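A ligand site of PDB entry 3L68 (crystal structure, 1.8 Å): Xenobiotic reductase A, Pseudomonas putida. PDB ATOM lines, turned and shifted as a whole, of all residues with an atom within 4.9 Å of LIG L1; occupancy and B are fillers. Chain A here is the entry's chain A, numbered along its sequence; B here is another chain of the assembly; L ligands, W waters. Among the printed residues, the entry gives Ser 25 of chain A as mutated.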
ATOM      1  N   PRO A  22     -26.445  22.497  25.906  1.00  0.00           N
ATOM      2  CA  PRO A  22     -26.043  21.108  25.670  1.00  0.00           C
ATOM      3  C   PRO A  22     -24.534  20.996  25.514  1.00  0.00           C
ATOM      4  O   PRO A  22     -23.859  22.018  25.350  1.00  0.00           O
ATOM      5  CB  PRO A  22     -26.738  20.758  24.348  1.00  0.00           C
ATOM      6  CG  PRO A  22     -26.887  22.087  23.638  1.00  0.00           C
ATOM      7  CD  PRO A  22     -26.940  23.160  24.687  1.00  0.00           C
ATOM      8  N   PRO A  23     -24.011  19.774  25.576  1.00  0.00           N
ATOM      9  CA  PRO A  23     -22.568  19.609  25.354  1.00  0.00           C
ATOM     10  C   PRO A  23     -22.202  20.132  23.978  1.00  0.00           C
ATOM     11  O   PRO A  23     -22.898  19.811  22.979  1.00  0.00           O
ATOM     12  CB  PRO A  23     -22.366  18.092  25.418  1.00  0.00           C
ATOM     13  CG  PRO A  23     -23.750  17.506  25.186  1.00  0.00           C
ATOM     14  CD  PRO A  23     -24.681  18.486  25.825  1.00  0.00           C
ATOM     15  N   MET A  24     -21.164  20.949  23.924  1.00  0.00           N
ATOM     16  CA  MET A  24     -20.604  21.440  22.678  1.00  0.00           C
ATOM     17  C   MET A  24     -19.064  21.369  22.709  1.00  0.00           C
ATOM     18  O   MET A  24     -18.397  22.216  23.306  1.00  0.00           O
ATOM     19  CB  MET A  24     -21.081  22.860  22.380  1.00  0.00           C
ATOM     20  CG  MET A  24     -22.501  22.927  21.823  1.00  0.00           C
ATOM     21  SD  MET A  24     -23.012  24.626  21.517  1.00  0.00           S
ATOM     22  CE  MET A  24     -22.970  25.301  23.176  1.00  0.00           C
ATOM     23  N   SER A  25     -18.536  20.351  22.046  1.00  0.00           N
ATOM     24  CA  SER A  25     -17.094  20.162  21.897  1.00  0.00           C
ATOM     25  C   SER A  25     -16.406  21.443  21.399  1.00  0.00           C
ATOM     26  O   SER A  25     -16.911  22.131  20.513  1.00  0.00           O
ATOM     27  CB  SER A  25     -16.823  19.015  20.924  1.00  0.00           C
ATOM     28  OG  SER A  25     -17.289  17.776  21.437  1.00  0.00           O
ATOM     29  N   GLU A  56     -18.948  19.679  27.347  1.00  0.00           N
ATOM     30  CA  GLU A  56     -18.782  18.942  26.090  1.00  0.00           C
ATOM     31  C   GLU A  56     -18.422  17.472  26.303  1.00  0.00           C
ATOM     32  O   GLU A  56     -17.957  17.092  27.376  1.00  0.00           O
ATOM     33  CB  GLU A  56     -17.666  19.576  25.277  1.00  0.00           C
ATOM     34  CG  GLU A  56     -16.308  19.466  25.954  1.00  0.00           C
ATOM     35  CD  GLU A  56     -15.312  20.491  25.456  1.00  0.00           C
ATOM     36  OE1 GLU A  56     -14.594  20.200  24.481  1.00  0.00           O
ATOM     37  OE2 GLU A  56     -15.258  21.595  26.031  1.00  0.00           O
ATOM     38  N   ALA A  57     -18.595  16.668  25.246  1.00  0.00           N
ATOM     39  CA  ALA A  57     -18.194  15.268  25.277  1.00  0.00           C
ATOM     40  C   ALA A  57     -16.783  15.126  25.838  1.00  0.00           C
ATOM     41  O   ALA A  57     -15.842  15.708  25.318  1.00  0.00           O
ATOM     42  CB  ALA A  57     -18.260  14.660  23.873  1.00  0.00           C
ATOM     43  N   GLN A  99     -20.983  15.649  29.953  1.00  0.00           N
ATOM     44  CA  GLN A  99     -21.246  14.487  29.117  1.00  0.00           C
ATOM     45  C   GLN A  99     -19.981  13.620  29.003  1.00  0.00           C
ATOM     46  O   GLN A  99     -18.940  14.103  28.574  1.00  0.00           O
ATOM     47  CB  GLN A  99     -21.689  14.917  27.721  1.00  0.00           C
ATOM     48  CG  GLN A  99     -22.008  13.752  26.801  1.00  0.00           C
ATOM     49  CD  GLN A  99     -22.233  14.187  25.372  1.00  0.00           C
ATOM     50  OE1 GLN A  99     -21.302  14.677  24.712  1.00  0.00           O
ATOM     51  NE2 GLN A  99     -23.450  14.026  24.876  1.00  0.00           N
ATOM     52  N   GLU A 176     -24.309  12.946  31.940  1.00  0.00           N
ATOM     53  CA  GLU A 176     -24.956  12.535  30.711  1.00  0.00           C
ATOM     54  C   GLU A 176     -24.106  11.517  29.966  1.00  0.00           C
ATOM     55  O   GLU A 176     -23.008  11.830  29.523  1.00  0.00           O
ATOM     56  CB  GLU A 176     -25.247  13.745  29.808  1.00  0.00           C
ATOM     57  CG  GLU A 176     -26.098  13.389  28.594  1.00  0.00           C
ATOM     58  CD  GLU A 176     -26.204  14.545  27.600  1.00  0.00           C
ATOM     59  OE1 GLU A 176     -27.020  15.460  27.838  1.00  0.00           O
ATOM     60  OE2 GLU A 176     -25.483  14.522  26.581  1.00  0.00           O
ATOM     61  N   HIS A 178     -23.066   9.547  26.812  1.00  0.00           N
ATOM     62  CA  HIS A 178     -23.182   9.842  25.373  1.00  0.00           C
ATOM     63  C   HIS A 178     -23.443   8.589  24.553  1.00  0.00           C
ATOM     64  O   HIS A 178     -22.500   7.981  24.018  1.00  0.00           O
ATOM     65  CB  HIS A 178     -21.922  10.527  24.849  1.00  0.00           C
ATOM     66  CG  HIS A 178     -22.138  11.258  23.555  1.00  0.00           C
ATOM     67  ND1 HIS A 178     -23.290  11.125  22.823  1.00  0.00           N
ATOM     68  CD2 HIS A 178     -21.348  12.131  22.876  1.00  0.00           C
ATOM     69  CE1 HIS A 178     -23.214  11.886  21.740  1.00  0.00           C
ATOM     70  NE2 HIS A 178     -22.046  12.505  21.752  1.00  0.00           N
ATOM     71  N   HIS A 181     -25.342   9.949  18.355  1.00  0.00           N
ATOM     72  CA  HIS A 181     -24.529  10.557  17.297  1.00  0.00           C
ATOM     73  C   HIS A 181     -23.498   9.612  16.653  1.00  0.00           C
ATOM     74  O   HIS A 181     -22.477  10.056  16.092  1.00  0.00           O
ATOM     75  CB  HIS A 181     -23.872  11.853  17.798  1.00  0.00           C
ATOM     76  CG  HIS A 181     -24.866  12.871  18.282  1.00  0.00           C
ATOM     77  ND1 HIS A 181     -24.497  13.968  19.051  1.00  0.00           N
ATOM     78  CD2 HIS A 181     -26.206  12.957  18.127  1.00  0.00           C
ATOM     79  CE1 HIS A 181     -25.578  14.688  19.328  1.00  0.00           C
ATOM     80  NE2 HIS A 181     -26.624  14.098  18.789  1.00  0.00           N
ATOM     81  N   ARG A 231     -27.779  10.751  26.466  1.00  0.00           N
ATOM     82  CA  ARG A 231     -28.175  11.224  25.155  1.00  0.00           C
ATOM     83  C   ARG A 231     -28.252  10.016  24.212  1.00  0.00           C
ATOM     84  O   ARG A 231     -27.373   9.168  24.220  1.00  0.00           O
ATOM     85  CB  ARG A 231     -27.195  12.275  24.623  1.00  0.00           C
ATOM     86  CG  ARG A 231     -27.776  13.093  23.445  1.00  0.00           C
ATOM     87  CD  ARG A 231     -26.969  14.367  23.135  1.00  0.00           C
ATOM     88  NE  ARG A 231     -27.854  15.403  22.577  1.00  0.00           N
ATOM     89  CZ  ARG A 231     -27.461  16.618  22.194  1.00  0.00           C
ATOM     90  NH1 ARG A 231     -28.360  17.475  21.707  1.00  0.00           N
ATOM     91  NH2 ARG A 231     -26.192  16.985  22.279  1.00  0.00           N
ATOM     92  N   ALA A 301     -32.806  19.259  21.025  1.00  0.00           N
ATOM     93  CA  ALA A 301     -32.152  20.429  20.493  1.00  0.00           C
ATOM     94  C   ALA A 301     -32.342  20.526  18.987  1.00  0.00           C
ATOM     95  O   ALA A 301     -32.902  19.618  18.357  1.00  0.00           O
ATOM     96  CB  ALA A 301     -30.642  20.413  20.845  1.00  0.00           C
ATOM     97  N   TRP A 302     -31.879  21.662  18.456  1.00  0.00           N
ATOM     98  CA  TRP A 302     -31.849  22.052  17.038  1.00  0.00           C
ATOM     99  C   TRP A 302     -32.870  23.130  16.691  1.00  0.00           C
ATOM    100  O   TRP A 302     -34.032  22.837  16.375  1.00  0.00           O
ATOM    101  CB  TRP A 302     -31.922  20.882  16.043  1.00  0.00           C
ATOM    102  CG  TRP A 302     -31.621  21.381  14.651  1.00  0.00           C
ATOM    103  CD1 TRP A 302     -32.482  22.024  13.796  1.00  0.00           C
ATOM    104  CD2 TRP A 302     -30.355  21.347  13.978  1.00  0.00           C
ATOM    105  NE1 TRP A 302     -31.841  22.357  12.633  1.00  0.00           N
ATOM    106  CE2 TRP A 302     -30.539  21.963  12.716  1.00  0.00           C
ATOM    107  CE3 TRP A 302     -29.089  20.855  14.308  1.00  0.00           C
ATOM    108  CZ2 TRP A 302     -29.492  22.084  11.792  1.00  0.00           C
ATOM    109  CZ3 TRP A 302     -28.064  20.978  13.394  1.00  0.00           C
ATOM    110  CH2 TRP A 302     -28.275  21.587  12.145  1.00  0.00           C
ATOM    111  N   GLY A 303     -32.424  24.381  16.736  1.00  0.00           N
ATOM    112  CA  GLY A 303     -33.208  25.515  16.308  1.00  0.00           C
ATOM    113  C   GLY A 303     -34.058  26.153  17.386  1.00  0.00           C
ATOM    114  O   GLY A 303     -34.984  26.901  17.095  1.00  0.00           O
ATOM    115  N   PHE A 304     -33.766  25.844  18.649  1.00  0.00           N
ATOM    116  CA  PHE A 304     -34.561  26.398  19.748  1.00  0.00           C
ATOM    117  C   PHE A 304     -34.002  27.724  20.252  1.00  0.00           C
ATOM    118  O   PHE A 304     -34.448  28.252  21.272  1.00  0.00           O
ATOM    119  CB  PHE A 304     -34.650  25.401  20.903  1.00  0.00           C
ATOM    120  CG  PHE A 304     -35.551  24.229  20.624  1.00  0.00           C
ATOM    121  CD1 PHE A 304     -36.920  24.316  20.813  1.00  0.00           C
ATOM    122  CD2 PHE A 304     -35.022  23.022  20.195  1.00  0.00           C
ATOM    123  CE1 PHE A 304     -37.742  23.231  20.567  1.00  0.00           C
ATOM    124  CE2 PHE A 304     -35.836  21.922  19.949  1.00  0.00           C
ATOM    125  CZ  PHE A 304     -37.204  22.030  20.129  1.00  0.00           C
ATOM    126  N   SER A 323     -32.789  22.547  25.122  1.00  0.00           N
ATOM    127  CA  SER A 323     -31.353  22.707  24.901  1.00  0.00           C
ATOM    128  C   SER A 323     -31.058  23.686  23.765  1.00  0.00           C
ATOM    129  O   SER A 323     -31.598  23.543  22.668  1.00  0.00           O
ATOM    130  CB  SER A 323     -30.726  21.347  24.587  1.00  0.00           C
ATOM    131  OG  SER A 323     -30.880  20.470  25.687  1.00  0.00           O
ATOM    132  N   VAL A 324     -30.205  24.655  24.043  1.00  0.00           N
ATOM    133  CA  VAL A 324     -29.890  25.740  23.109  1.00  0.00           C
ATOM    134  C   VAL A 324     -28.375  25.831  22.955  1.00  0.00           C
ATOM    135  O   VAL A 324     -27.676  26.234  23.894  1.00  0.00           O
ATOM    136  CB  VAL A 324     -30.427  27.078  23.638  1.00  0.00           C
ATOM    137  CG1 VAL A 324     -30.048  28.228  22.676  1.00  0.00           C
ATOM    138  CG2 VAL A 324     -31.942  27.000  23.799  1.00  0.00           C
ATOM    139  N   GLY A 325     -27.881  25.432  21.793  1.00  0.00           N
ATOM    140  CA  GLY A 325     -26.450  25.261  21.567  1.00  0.00           C
ATOM    141  C   GLY A 325     -25.789  26.428  20.854  1.00  0.00           C
ATOM    142  O   GLY A 325     -25.209  27.313  21.480  1.00  0.00           O
ATOM    143  N   ARG A 326     -25.875  26.435  19.525  1.00  0.00           N
ATOM    144  CA  ARG A 326     -25.201  27.458  18.734  1.00  0.00           C
ATOM    145  C   ARG A 326     -25.564  28.889  19.112  1.00  0.00           C
ATOM    146  O   ARG A 326     -24.723  29.778  19.057  1.00  0.00           O
ATOM    147  CB  ARG A 326     -25.398  27.206  17.230  1.00  0.00           C
ATOM    148  CG  ARG A 326     -24.536  26.062  16.723  1.00  0.00           C
ATOM    149  CD  ARG A 326     -24.960  25.574  15.375  1.00  0.00           C
ATOM    150  NE  ARG A 326     -26.307  25.013  15.416  1.00  0.00           N
ATOM    151  CZ  ARG A 326     -26.946  24.518  14.367  1.00  0.00           C
ATOM    152  NH1 ARG A 326     -26.346  24.505  13.184  1.00  0.00           N
ATOM    153  NH2 ARG A 326     -28.177  24.021  14.500  1.00  0.00           N
ATOM    154  N   ALA A 327     -26.811  29.122  19.533  1.00  0.00           N
ATOM    155  CA  ALA A 327     -27.185  30.482  19.937  1.00  0.00           C
ATOM    156  C   ALA A 327     -26.298  30.981  21.084  1.00  0.00           C
ATOM    157  O   ALA A 327     -26.085  32.176  21.238  1.00  0.00           O
ATOM    158  CB  ALA A 327     -28.664  30.548  20.319  1.00  0.00           C
ATOM    159  N   LEU A 329     -23.072  30.138  21.474  1.00  0.00           N
ATOM    160  CA  LEU A 329     -21.748  30.435  20.962  1.00  0.00           C
ATOM    161  C   LEU A 329     -21.783  31.843  20.373  1.00  0.00           C
ATOM    162  O   LEU A 329     -20.817  32.594  20.492  1.00  0.00           O
ATOM    163  CB  LEU A 329     -21.309  29.418  19.919  1.00  0.00           C
ATOM    164  CG  LEU A 329     -21.368  27.933  20.311  1.00  0.00           C
ATOM    165  CD1 LEU A 329     -21.064  27.048  19.103  1.00  0.00           C
ATOM    166  CD2 LEU A 329     -20.418  27.601  21.480  1.00  0.00           C
ATOM    167  N   PRO B 354     -13.430  27.939  17.616  1.00  0.00           N
ATOM    168  CA  PRO B 354     -14.426  27.018  18.205  1.00  0.00           C
ATOM    169  C   PRO B 354     -15.838  27.584  18.203  1.00  0.00           C
ATOM    170  O   PRO B 354     -16.783  26.848  18.490  1.00  0.00           O
ATOM    171  CB  PRO B 354     -13.942  26.822  19.645  1.00  0.00           C
ATOM    172  CG  PRO B 354     -12.477  27.088  19.582  1.00  0.00           C
ATOM    173  CD  PRO B 354     -12.318  28.200  18.554  1.00  0.00           C
ATOM    174  N   TRP B 358     -18.924  27.399  13.372  1.00  0.00           N
ATOM    175  CA  TRP B 358     -20.299  26.889  13.424  1.00  0.00           C
ATOM    176  C   TRP B 358     -21.343  27.940  13.126  1.00  0.00           C
ATOM    177  O   TRP B 358     -22.520  27.628  12.971  1.00  0.00           O
ATOM    178  CB  TRP B 358     -20.584  26.277  14.802  1.00  0.00           C
ATOM    179  CG  TRP B 358     -19.520  25.343  15.209  1.00  0.00           C
ATOM    180  CD1 TRP B 358     -18.501  25.589  16.085  1.00  0.00           C
ATOM    181  CD2 TRP B 358     -19.315  24.017  14.713  1.00  0.00           C
ATOM    182  NE1 TRP B 358     -17.684  24.487  16.182  1.00  0.00           N
ATOM    183  CE2 TRP B 358     -18.163  23.510  15.346  1.00  0.00           C
ATOM    184  CE3 TRP B 358     -19.999  23.210  13.803  1.00  0.00           C
ATOM    185  CZ2 TRP B 358     -17.689  22.219  15.108  1.00  0.00           C
ATOM    186  CZ3 TRP B 358     -19.527  21.931  13.558  1.00  0.00           C
ATOM    187  CH2 TRP B 358     -18.382  21.452  14.199  1.00  0.00           C
HETATM  188  N1  LIG L   1     -23.509  17.090  20.957  1.00  0.00           N
HETATM  189  C1  LIG L   1     -23.053  16.117  21.816  1.00  0.00           C
HETATM  190  O1  LIG L   1     -23.807  15.206  22.159  1.00  0.00           O
HETATM  191  N2  LIG L   1     -21.760  16.142  22.294  1.00  0.00           N
HETATM  192  C2  LIG L   1     -20.908  17.167  21.910  1.00  0.00           C
HETATM  193  O2  LIG L   1     -19.749  17.214  22.347  1.00  0.00           O
HETATM  194  C3  LIG L   1     -21.367  18.152  21.043  1.00  0.00           C
HETATM  195  N3  LIG L   1     -20.525  19.159  20.661  1.00  0.00           N
HETATM  196  C4  LIG L   1     -20.981  20.144  19.808  1.00  0.00           C
HETATM  197  C5  LIG L   1     -20.115  21.162  19.435  1.00  0.00           C
HETATM  198  C6  LIG L   1     -20.545  22.167  18.577  1.00  0.00           C
HETATM  199  C7  LIG L   1     -19.573  23.254  18.212  1.00  0.00           C
HETATM  200  C8  LIG L   1     -21.843  22.153  18.078  1.00  0.00           C
HETATM  201  C9  LIG L   1     -22.302  23.244  17.152  1.00  0.00           C
HETATM  202  C10 LIG L   1     -22.714  21.126  18.452  1.00  0.00           C
HETATM  203  C11 LIG L   1     -22.282  20.109  19.317  1.00  0.00           C
HETATM  204  N4  LIG L   1     -23.129  19.081  19.694  1.00  0.00           N
HETATM  205  C12 LIG L   1     -22.675  18.112  20.575  1.00  0.00           C
HETATM  206  C13 LIG L   1     -24.563  19.039  19.214  1.00  0.00           C
HETATM  207  C14 LIG L   1     -25.268  20.067  20.105  1.00  0.00           C
HETATM  208  O3  LIG L   1     -25.218  19.612  21.437  1.00  0.00           O
HETATM  209  C15 LIG L   1     -26.713  20.369  19.676  1.00  0.00           C
HETATM  210  O4  LIG L   1     -27.502  19.190  19.643  1.00  0.00           O
HETATM  211  C16 LIG L   1     -26.761  21.021  18.281  1.00  0.00           C
HETATM  212  O5  LIG L   1     -25.886  22.140  18.206  1.00  0.00           O
HETATM  213  C17 LIG L   1     -28.177  21.475  17.914  1.00  0.00           C
HETATM  214  O6  LIG L   1     -28.630  22.511  18.765  1.00  0.00           O
HETATM  215  P1  LIG L   1     -28.585  24.059  18.274  1.00  0.00           P
HETATM  216  O7  LIG L   1     -27.138  24.417  18.046  1.00  0.00           O
HETATM  217  O8  LIG L   1     -29.320  24.259  16.981  1.00  0.00           O
HETATM  218  O9  LIG L   1     -29.191  24.930  19.344  1.00  0.00           O
HETATM  219  C1  LG2 L   2     -21.223  15.487  18.987  1.00  0.00           C
HETATM  220  C2  LG2 L   2     -19.896  15.857  19.155  1.00  0.00           C
HETATM  221  C3  LG2 L   2     -19.377  16.912  18.407  1.00  0.00           C
HETATM  222  C4  LG2 L   2     -20.203  17.563  17.495  1.00  0.00           C
HETATM  223  C5  LG2 L   2     -19.716  18.624  16.738  1.00  0.00           C
HETATM  224  C6  LG2 L   2     -20.546  19.278  15.834  1.00  0.00           C
HETATM  225  C7  LG2 L   2     -21.867  18.885  15.679  1.00  0.00           C
HETATM  226  C8  LG2 L   2     -22.359  17.828  16.444  1.00  0.00           C
HETATM  227  C9  LG2 L   2     -21.529  17.174  17.348  1.00  0.00           C
HETATM  228  O1  LG2 L   2     -21.706  14.538  19.646  1.00  0.00           O
HETATM  229  O2  LG2 L   2     -22.024  16.137  18.077  1.00  0.00           O
HETATM  230  O   HOH W   1     -29.702  26.534  15.695  1.00  0.00           O
HETATM  231  O   HOH W   2     -31.551  24.058  19.941  1.00  0.00           O
HETATM  232  O   HOH W   3     -29.152  27.592  19.150  1.00  0.00           O
HETATM  233  O   HOH W   4     -25.224  21.501  15.565  1.00  0.00           O
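Water W1 bridges an oxygen (O8) of LIG L1 (2.6 Å) and the guanidinium group of Arg 326 (3.2 Å). Water W3 lies within hydrogen-bond range of O9 of LIG L1, N of Ala 327 and N of Arg 326.
O1 of LG2 L2 sits close to N2 of LIG L1.
The side-chain amide oxygen (OE1) of Gln 99 sits close to the backbone NH (N) of Ala 57 (3.4 Å). The side-chain carboxylate (OE2) of Glu 176 sits at hydrogen-bond distance from the side-chain amide nitrogen (NE2) of Gln 99 (2.7 Å). The indole nitrogen (NE1) of Trp 358 of chain B lies close to the backbone carbonyl oxygen (O) of Pro 354 of chain B.
Merely in contact with LIG L1: Trp 358 of chain B (3.0 Å), Met 24 (3.0 Å), Pro 22 (3.5 Å), Ala 301 (3.6 Å) and Val 324 (3.8 Å). Hydrophobic or aromatic side chains within 4 Å of LIG L1: Pro 22, Pro 23, Met 24, Ala 57, His 178, His 181, Ala 301, Trp 302 and Trp 358 of chain B. 16 residues have an atom within 4 Å of LIG L1: Pro 22, Pro 23, Met 24, Ser 25, Ala 57, Gln 99, His 178, His 181, Arg 231, Ala 301, Trp 302, Gly 303, Val 324, Gly 325, Arg 326 and Trp 358 of chain B. The nearest printed residue that does not touch LIG L1 is Leu 329 (4.2 Å).
The backbone NH (N) of Ser 25 lies within hydrogen-bond range of a nitrogen (N3) of LIG L1. O2 of LIG L1 sits at hydrogen-bond distance from OG of Ser 25, 2.7 Å away. An oxygen (O7) of LIG L1 sits at hydrogen-bond distance from the backbone NH of Arg 326 (2.8 Å). The guanidinium group of Arg 326 is in salt-bridge range of an oxygen (O8) of LIG L1, at 2.7 Å. The backbone carbonyl oxygen (O) of Pro 23 is in hydrogen-bond range of an oxygen (O3) of LIG L1 (2.8 Å). An oxygen (O4) of LIG L1 is in hydrogen-bond range of the guanidinium group of Arg 231 (2.8 Å). An oxygen (O9) of LIG L1 is in hydrogen-bond range of the backbone NH (N) of Gly 325 (2.8 Å). A nitrogen (N2) of LIG L1 lies within hydrogen-bond range of the side-chain amide oxygen (OE1) of Gln 99 (2.9 Å). The backbone NH (N) of Gly 303 is in hydrogen-bond range of an oxygen (O8) of LIG L1. O2 of LIG L1 sits at hydrogen-bond distance from N of Ala 57 (3.2 Å). NE2 of His 178 lies within hydrogen-bond range of O1 of LIG L1, 3.2 Å away. N of Trp 302 sits at hydrogen-bond distance from O6 of LIG L1 (3.4 Å). An oxygen (O1) of LIG L1 sits close to a ring nitrogen (ND1) of His 181, at 3.4 Å. A ring nitrogen (NE2) of His 178 is in hydrogen-bond range of an oxygen (O1) of LG2 L2 (2.9 Å). An oxygen (O1) of LG2 L2 is in hydrogen-bond range of a ring nitrogen (ND1) of His 181 (2.9 Å).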
